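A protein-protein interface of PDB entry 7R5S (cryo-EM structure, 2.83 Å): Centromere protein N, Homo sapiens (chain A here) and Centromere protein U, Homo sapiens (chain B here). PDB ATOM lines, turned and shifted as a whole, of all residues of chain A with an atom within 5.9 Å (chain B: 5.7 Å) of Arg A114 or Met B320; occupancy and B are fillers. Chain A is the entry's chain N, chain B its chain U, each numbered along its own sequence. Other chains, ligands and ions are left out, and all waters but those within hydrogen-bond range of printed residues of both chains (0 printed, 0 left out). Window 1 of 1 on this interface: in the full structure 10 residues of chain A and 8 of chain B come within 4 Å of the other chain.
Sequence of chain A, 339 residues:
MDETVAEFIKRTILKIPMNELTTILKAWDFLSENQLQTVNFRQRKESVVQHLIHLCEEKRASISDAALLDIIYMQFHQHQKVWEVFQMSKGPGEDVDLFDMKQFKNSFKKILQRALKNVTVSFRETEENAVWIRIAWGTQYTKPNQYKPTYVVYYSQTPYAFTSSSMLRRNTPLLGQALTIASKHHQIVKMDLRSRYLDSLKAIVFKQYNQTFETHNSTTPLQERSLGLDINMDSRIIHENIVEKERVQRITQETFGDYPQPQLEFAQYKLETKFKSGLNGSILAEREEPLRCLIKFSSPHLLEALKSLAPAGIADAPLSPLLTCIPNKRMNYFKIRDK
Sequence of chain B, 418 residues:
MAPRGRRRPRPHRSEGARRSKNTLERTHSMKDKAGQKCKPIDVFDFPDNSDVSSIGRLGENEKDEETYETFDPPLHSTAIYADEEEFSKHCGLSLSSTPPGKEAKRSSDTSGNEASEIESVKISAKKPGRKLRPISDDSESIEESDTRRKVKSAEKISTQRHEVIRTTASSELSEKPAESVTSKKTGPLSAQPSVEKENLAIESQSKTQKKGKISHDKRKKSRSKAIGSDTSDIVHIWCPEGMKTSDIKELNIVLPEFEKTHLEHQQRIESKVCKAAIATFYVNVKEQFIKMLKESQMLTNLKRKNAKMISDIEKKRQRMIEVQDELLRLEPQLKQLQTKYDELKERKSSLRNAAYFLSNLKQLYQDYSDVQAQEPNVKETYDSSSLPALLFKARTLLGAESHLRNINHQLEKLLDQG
Among the printed residues, pairs that only touch across the chains: Leu A116 with Arg B317 and Gln A177 with Gln B324.
The guanidinium group (NH2) of Arg B317 lies within hydrogen-bond range of the side-chain amide oxygen (OE1) of Gln A140, 2.9 Å away. SD of Met B320 lies within hydrogen-bond range of NH1 of Arg A114 (3.6 Å). The side-chain amide oxygen (OE1) of Gln B324 lies within hydrogen-bond range of the guanidinium group (NH2) of Arg A114, 3.3 Å away. The side-chain amide nitrogen (NE2) of Gln A177 lies close to the backbone NH (N) of Asp B325, 3.2 Å away. The side-chain amide nitrogen (NE2) of Gln A177 sits at hydrogen-bond distance from the backbone carbonyl oxygen (O) of Ile B321 (2.9 Å).
Hydrophobic or aromatic side chains of chain A within 4 Å of the printed part of chain B: Leu A116. Of the 10 printed residues of chain B, 5 touch a printed residue of chain A. Hydrophobic or aromatic side chains of chain B within 4 Å of the printed part of chain A: Met B320. Among the printed residues, no Asp or Glu carboxylate lies within 4 Å of a Lys or Arg side-chain nitrogen of the other chain.
Of chain B, only Met B320 (3.6 Å) and Gln B324 (3.3 Å) come within 4 Å of Arg A114. Of chain A, only Arg A114 comes within 4 Å of Met B320. Of the printed residues of chain A, Gln B324 touches Arg A114 (3.3 Å) and Gln A177 (3.3 Å). Of the printed residues of chain A, Arg B317 touches Leu A116 (3.4 Å) and Gln A140 (2.9 Å). Lys A109 touches none of the printed residues of chain B. Lys B316 touches none of the printed residues of chain A. The nearest printed residue of chain B that does not touch Arg A114 is Ile B321 (6.5 Å). The nearest residue of chain A that does not touch Met B320 is Ala A115 (4.3 Å).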
ATOM      1  N   LYS A 109     -10.316  -2.581 -17.086  1.00  0.00           N
ATOM      2  CA  LYS A 109      -9.474  -3.312 -18.023  1.00  0.00           C
ATOM      3  C   LYS A 109     -10.283  -3.853 -19.196  1.00  0.00           C
ATOM      4  O   LYS A 109      -9.840  -3.765 -20.347  1.00  0.00           O
ATOM      5  CB  LYS A 109      -8.751  -4.449 -17.300  1.00  0.00           C
ATOM      6  CG  LYS A 109      -7.747  -5.195 -18.161  1.00  0.00           C
ATOM      7  CD  LYS A 109      -7.054  -6.291 -17.368  1.00  0.00           C
ATOM      8  CE  LYS A 109      -6.375  -5.730 -16.131  1.00  0.00           C
ATOM      9  NZ  LYS A 109      -5.715  -6.796 -15.327  1.00  0.00           N
ATOM     10  N   LYS A 110     -11.472  -4.400 -18.926  1.00  0.00           N
ATOM     11  CA  LYS A 110     -12.265  -5.019 -19.984  1.00  0.00           C
ATOM     12  C   LYS A 110     -12.769  -3.989 -20.985  1.00  0.00           C
ATOM     13  O   LYS A 110     -12.868  -4.283 -22.181  1.00  0.00           O
ATOM     14  CB  LYS A 110     -13.436  -5.793 -19.379  1.00  0.00           C
ATOM     15  CG  LYS A 110     -13.040  -7.094 -18.702  1.00  0.00           C
ATOM     16  CD  LYS A 110     -12.386  -8.050 -19.684  1.00  0.00           C
ATOM     17  CE  LYS A 110     -11.950  -9.333 -18.993  1.00  0.00           C
ATOM     18  NZ  LYS A 110     -13.085 -10.003 -18.304  1.00  0.00           N
ATOM     19  N   ILE A 111     -13.093  -2.778 -20.523  1.00  0.00           N
ATOM     20  CA  ILE A 111     -13.564  -1.745 -21.446  1.00  0.00           C
ATOM     21  C   ILE A 111     -12.494  -1.439 -22.489  1.00  0.00           C
ATOM     22  O   ILE A 111     -12.757  -1.443 -23.699  1.00  0.00           O
ATOM     23  CB  ILE A 111     -13.981  -0.481 -20.674  1.00  0.00           C
ATOM     24  CG1 ILE A 111     -15.266  -0.738 -19.886  1.00  0.00           C
ATOM     25  CG2 ILE A 111     -14.172   0.686 -21.629  1.00  0.00           C
ATOM     26  CD1 ILE A 111     -16.441  -1.135 -20.748  1.00  0.00           C
ATOM     27  N   LEU A 112     -11.265  -1.186 -22.035  1.00  0.00           N
ATOM     28  CA  LEU A 112     -10.182  -0.885 -22.965  1.00  0.00           C
ATOM     29  C   LEU A 112      -9.763  -2.110 -23.767  1.00  0.00           C
ATOM     30  O   LEU A 112      -9.277  -1.971 -24.894  1.00  0.00           O
ATOM     31  CB  LEU A 112      -8.984  -0.311 -22.208  1.00  0.00           C
ATOM     32  CG  LEU A 112      -9.235   0.964 -21.401  1.00  0.00           C
ATOM     33  CD1 LEU A 112      -7.955   1.431 -20.726  1.00  0.00           C
ATOM     34  CD2 LEU A 112      -9.804   2.059 -22.286  1.00  0.00           C
ATOM     35  N   GLN A 113      -9.937  -3.313 -23.211  1.00  0.00           N
ATOM     36  CA  GLN A 113      -9.570  -4.517 -23.947  1.00  0.00           C
ATOM     37  C   GLN A 113     -10.563  -4.824 -25.060  1.00  0.00           C
ATOM     38  O   GLN A 113     -10.182  -5.405 -26.082  1.00  0.00           O
ATOM     39  CB  GLN A 113      -9.460  -5.706 -22.993  1.00  0.00           C
ATOM     40  CG  GLN A 113      -8.158  -5.760 -22.209  1.00  0.00           C
ATOM     41  CD  GLN A 113      -6.960  -6.081 -23.081  1.00  0.00           C
ATOM     42  OE1 GLN A 113      -7.102  -6.612 -24.182  1.00  0.00           O
ATOM     43  NE2 GLN A 113      -5.770  -5.759 -22.590  1.00  0.00           N
ATOM     44  N   ARG A 114     -11.830  -4.456 -24.882  1.00  0.00           N
ATOM     45  CA  ARG A 114     -12.822  -4.676 -25.927  1.00  0.00           C
ATOM     46  C   ARG A 114     -12.898  -3.522 -26.914  1.00  0.00           C
ATOM     47  O   ARG A 114     -13.294  -3.730 -28.067  1.00  0.00           O
ATOM     48  CB  ARG A 114     -14.204  -4.923 -25.314  1.00  0.00           C
ATOM     49  CG  ARG A 114     -14.876  -3.688 -24.741  1.00  0.00           C
ATOM     50  CD  ARG A 114     -16.381  -3.882 -24.636  1.00  0.00           C
ATOM     51  NE  ARG A 114     -17.049  -2.710 -24.080  1.00  0.00           N
ATOM     52  CZ  ARG A 114     -17.351  -1.619 -24.777  1.00  0.00           C
ATOM     53  NH1 ARG A 114     -17.045  -1.547 -26.065  1.00  0.00           N
ATOM     54  NH2 ARG A 114     -17.960  -0.601 -24.187  1.00  0.00           N
ATOM     55  N   ALA A 115     -12.528  -2.308 -26.498  1.00  0.00           N
ATOM     56  CA  ALA A 115     -12.502  -1.189 -27.434  1.00  0.00           C
ATOM     57  C   ALA A 115     -11.291  -1.278 -28.355  1.00  0.00           C
ATOM     58  O   ALA A 115     -11.430  -1.377 -29.579  1.00  0.00           O
ATOM     59  CB  ALA A 115     -12.507   0.135 -26.669  1.00  0.00           C
ATOM     60  N   LEU A 116     -10.092  -1.242 -27.782  1.00  0.00           N
ATOM     61  CA  LEU A 116      -8.863  -1.414 -28.538  1.00  0.00           C
ATOM     62  C   LEU A 116      -8.477  -2.892 -28.534  1.00  0.00           C
ATOM     63  O   LEU A 116      -9.252  -3.756 -28.115  1.00  0.00           O
ATOM     64  CB  LEU A 116      -7.761  -0.529 -27.959  1.00  0.00           C
ATOM     65  CG  LEU A 116      -8.063   0.968 -27.887  1.00  0.00           C
ATOM     66  CD1 LEU A 116      -6.971   1.703 -27.129  1.00  0.00           C
ATOM     67  CD2 LEU A 116      -8.232   1.548 -29.282  1.00  0.00           C
ATOM     68  N   GLN A 140      -5.263  -2.225 -33.137  1.00  0.00           N
ATOM     69  CA  GLN A 140      -5.262  -3.576 -33.686  1.00  0.00           C
ATOM     70  C   GLN A 140      -4.052  -3.861 -34.566  1.00  0.00           C
ATOM     71  O   GLN A 140      -3.741  -5.034 -34.803  1.00  0.00           O
ATOM     72  CB  GLN A 140      -6.543  -3.819 -34.488  1.00  0.00           C
ATOM     73  CG  GLN A 140      -7.799  -3.987 -33.645  1.00  0.00           C
ATOM     74  CD  GLN A 140      -8.344  -2.672 -33.125  1.00  0.00           C
ATOM     75  OE1 GLN A 140      -7.842  -1.601 -33.461  1.00  0.00           O
ATOM     76  NE2 GLN A 140      -9.380  -2.748 -32.297  1.00  0.00           N
ATOM     77  N   GLN A 177     -15.324   7.173 -21.041  1.00  0.00           N
ATOM     78  CA  GLN A 177     -16.280   6.075 -20.954  1.00  0.00           C
ATOM     79  C   GLN A 177     -15.811   5.011 -19.972  1.00  0.00           C
ATOM     80  O   GLN A 177     -16.600   4.514 -19.159  1.00  0.00           O
ATOM     81  CB  GLN A 177     -16.498   5.460 -22.335  1.00  0.00           C
ATOM     82  CG  GLN A 177     -17.754   5.926 -23.043  1.00  0.00           C
ATOM     83  CD  GLN A 177     -18.061   5.095 -24.271  1.00  0.00           C
ATOM     84  OE1 GLN A 177     -17.260   4.256 -24.683  1.00  0.00           O
ATOM     85  NE2 GLN A 177     -19.225   5.323 -24.865  1.00  0.00           N
ATOM     86  N   LYS B 316     -15.132   2.134 -37.730  1.00  0.00           N
ATOM     87  CA  LYS B 316     -16.101   1.408 -36.910  1.00  0.00           C
ATOM     88  C   LYS B 316     -15.905   1.661 -35.419  1.00  0.00           C
ATOM     89  O   LYS B 316     -16.858   1.524 -34.633  1.00  0.00           O
ATOM     90  CB  LYS B 316     -16.015  -0.091 -37.201  1.00  0.00           C
ATOM     91  CG  LYS B 316     -16.541  -0.495 -38.568  1.00  0.00           C
ATOM     92  CD  LYS B 316     -18.054  -0.389 -38.632  1.00  0.00           C
ATOM     93  CE  LYS B 316     -18.591  -0.949 -39.939  1.00  0.00           C
ATOM     94  NZ  LYS B 316     -20.078  -0.918 -39.988  1.00  0.00           N
ATOM     95  N   ARG B 317     -14.678   1.997 -35.006  1.00  0.00           N
ATOM     96  CA  ARG B 317     -14.425   2.262 -33.590  1.00  0.00           C
ATOM     97  C   ARG B 317     -15.321   3.379 -33.054  1.00  0.00           C
ATOM     98  O   ARG B 317     -15.899   3.258 -31.962  1.00  0.00           O
ATOM     99  CB  ARG B 317     -12.952   2.610 -33.382  1.00  0.00           C
ATOM    100  CG  ARG B 317     -12.488   2.543 -31.939  1.00  0.00           C
ATOM    101  CD  ARG B 317     -10.999   2.826 -31.836  1.00  0.00           C
ATOM    102  NE  ARG B 317     -10.219   1.957 -32.711  1.00  0.00           N
ATOM    103  CZ  ARG B 317      -8.915   2.096 -32.933  1.00  0.00           C
ATOM    104  NH1 ARG B 317      -8.242   3.076 -32.347  1.00  0.00           N
ATOM    105  NH2 ARG B 317      -8.286   1.258 -33.745  1.00  0.00           N
ATOM    106  N   GLN B 318     -15.451   4.474 -33.808  1.00  0.00           N
ATOM    107  CA  GLN B 318     -16.260   5.601 -33.349  1.00  0.00           C
ATOM    108  C   GLN B 318     -17.736   5.229 -33.273  1.00  0.00           C
ATOM    109  O   GLN B 318     -18.452   5.689 -32.374  1.00  0.00           O
ATOM    110  CB  GLN B 318     -16.057   6.802 -34.272  1.00  0.00           C
ATOM    111  CG  GLN B 318     -14.619   7.285 -34.354  1.00  0.00           C
ATOM    112  CD  GLN B 318     -14.462   8.488 -35.262  1.00  0.00           C
ATOM    113  OE1 GLN B 318     -15.445   9.039 -35.758  1.00  0.00           O
ATOM    114  NE2 GLN B 318     -13.221   8.904 -35.485  1.00  0.00           N
ATOM    115  N   ARG B 319     -18.211   4.411 -34.214  1.00  0.00           N
ATOM    116  CA  ARG B 319     -19.588   3.930 -34.150  1.00  0.00           C
ATOM    117  C   ARG B 319     -19.824   3.123 -32.881  1.00  0.00           C
ATOM    118  O   ARG B 319     -20.847   3.296 -32.204  1.00  0.00           O
ATOM    119  CB  ARG B 319     -19.906   3.094 -35.389  1.00  0.00           C
ATOM    120  CG  ARG B 319     -21.232   2.358 -35.324  1.00  0.00           C
ATOM    121  CD  ARG B 319     -22.404   3.316 -35.440  1.00  0.00           C
ATOM    122  NE  ARG B 319     -23.684   2.621 -35.347  1.00  0.00           N
ATOM    123  CZ  ARG B 319     -24.285   2.023 -36.371  1.00  0.00           C
ATOM    124  NH1 ARG B 319     -23.722   2.033 -37.571  1.00  0.00           N
ATOM    125  NH2 ARG B 319     -25.450   1.415 -36.195  1.00  0.00           N
ATOM    126  N   MET B 320     -18.888   2.233 -32.546  1.00  0.00           N
ATOM    127  CA  MET B 320     -19.005   1.480 -31.298  1.00  0.00           C
ATOM    128  C   MET B 320     -19.077   2.417 -30.097  1.00  0.00           C
ATOM    129  O   MET B 320     -19.926   2.250 -29.206  1.00  0.00           O
ATOM    130  CB  MET B 320     -17.829   0.514 -31.154  1.00  0.00           C
ATOM    131  CG  MET B 320     -17.673  -0.056 -29.754  1.00  0.00           C
ATOM    132  SD  MET B 320     -16.231  -1.121 -29.587  1.00  0.00           S
ATOM    133  CE  MET B 320     -16.645  -2.416 -30.750  1.00  0.00           C
ATOM    134  N   ILE B 321     -18.190   3.415 -30.061  1.00  0.00           N
ATOM    135  CA  ILE B 321     -18.154   4.343 -28.932  1.00  0.00           C
ATOM    136  C   ILE B 321     -19.480   5.086 -28.799  1.00  0.00           C
ATOM    137  O   ILE B 321     -20.030   5.219 -27.695  1.00  0.00           O
ATOM    138  CB  ILE B 321     -16.970   5.318 -29.080  1.00  0.00           C
ATOM    139  CG1 ILE B 321     -15.644   4.570 -28.939  1.00  0.00           C
ATOM    140  CG2 ILE B 321     -17.067   6.439 -28.057  1.00  0.00           C
ATOM    141  CD1 ILE B 321     -14.427   5.466 -29.010  1.00  0.00           C
ATOM    142  N   GLU B 322     -20.022   5.576 -29.918  1.00  0.00           N
ATOM    143  CA  GLU B 322     -21.251   6.361 -29.841  1.00  0.00           C
ATOM    144  C   GLU B 322     -22.453   5.495 -29.480  1.00  0.00           C
ATOM    145  O   GLU B 322     -23.358   5.960 -28.776  1.00  0.00           O
ATOM    146  CB  GLU B 322     -21.490   7.112 -31.153  1.00  0.00           C
ATOM    147  CG  GLU B 322     -21.857   6.245 -32.343  1.00  0.00           C
ATOM    148  CD  GLU B 322     -21.968   7.040 -33.629  1.00  0.00           C
ATOM    149  OE1 GLU B 322     -21.473   8.186 -33.665  1.00  0.00           O
ATOM    150  OE2 GLU B 322     -22.552   6.520 -34.603  1.00  0.00           O
ATOM    151  N   VAL B 323     -22.478   4.232 -29.917  1.00  0.00           N
ATOM    152  CA  VAL B 323     -23.580   3.363 -29.512  1.00  0.00           C
ATOM    153  C   VAL B 323     -23.504   3.062 -28.017  1.00  0.00           C
ATOM    154  O   VAL B 323     -24.538   3.022 -27.326  1.00  0.00           O
ATOM    155  CB  VAL B 323     -23.589   2.074 -30.353  1.00  0.00           C
ATOM    156  CG1 VAL B 323     -24.621   1.097 -29.821  1.00  0.00           C
ATOM    157  CG2 VAL B 323     -23.877   2.397 -31.810  1.00  0.00           C
ATOM    158  N   GLN B 324     -22.294   2.858 -27.489  1.00  0.00           N
ATOM    159  CA  GLN B 324     -22.149   2.677 -26.046  1.00  0.00           C
ATOM    160  C   GLN B 324     -22.635   3.908 -25.288  1.00  0.00           C
ATOM    161  O   GLN B 324     -23.335   3.788 -24.271  1.00  0.00           O
ATOM    162  CB  GLN B 324     -20.693   2.368 -25.697  1.00  0.00           C
ATOM    163  CG  GLN B 324     -20.409   2.310 -24.204  1.00  0.00           C
ATOM    164  CD  GLN B 324     -21.273   1.299 -23.482  1.00  0.00           C
ATOM    165  OE1 GLN B 324     -21.104   0.091 -23.644  1.00  0.00           O
ATOM    166  NE2 GLN B 324     -22.209   1.788 -22.676  1.00  0.00           N
ATOM    167  N   ASP B 325     -22.267   5.101 -25.769  1.00  0.00           N
ATOM    168  CA  ASP B 325     -22.751   6.333 -25.148  1.00  0.00           C
ATOM    169  C   ASP B 325     -24.274   6.401 -25.162  1.00  0.00           C
ATOM    170  O   ASP B 325     -24.897   6.783 -24.162  1.00  0.00           O
ATOM    171  CB  ASP B 325     -22.162   7.550 -25.861  1.00  0.00           C
ATOM    172  CG  ASP B 325     -20.820   7.967 -25.296  1.00  0.00           C
ATOM    173  OD1 ASP B 325     -19.795   7.377 -25.696  1.00  0.00           O
ATOM    174  OD2 ASP B 325     -20.790   8.887 -24.452  1.00  0.00           O
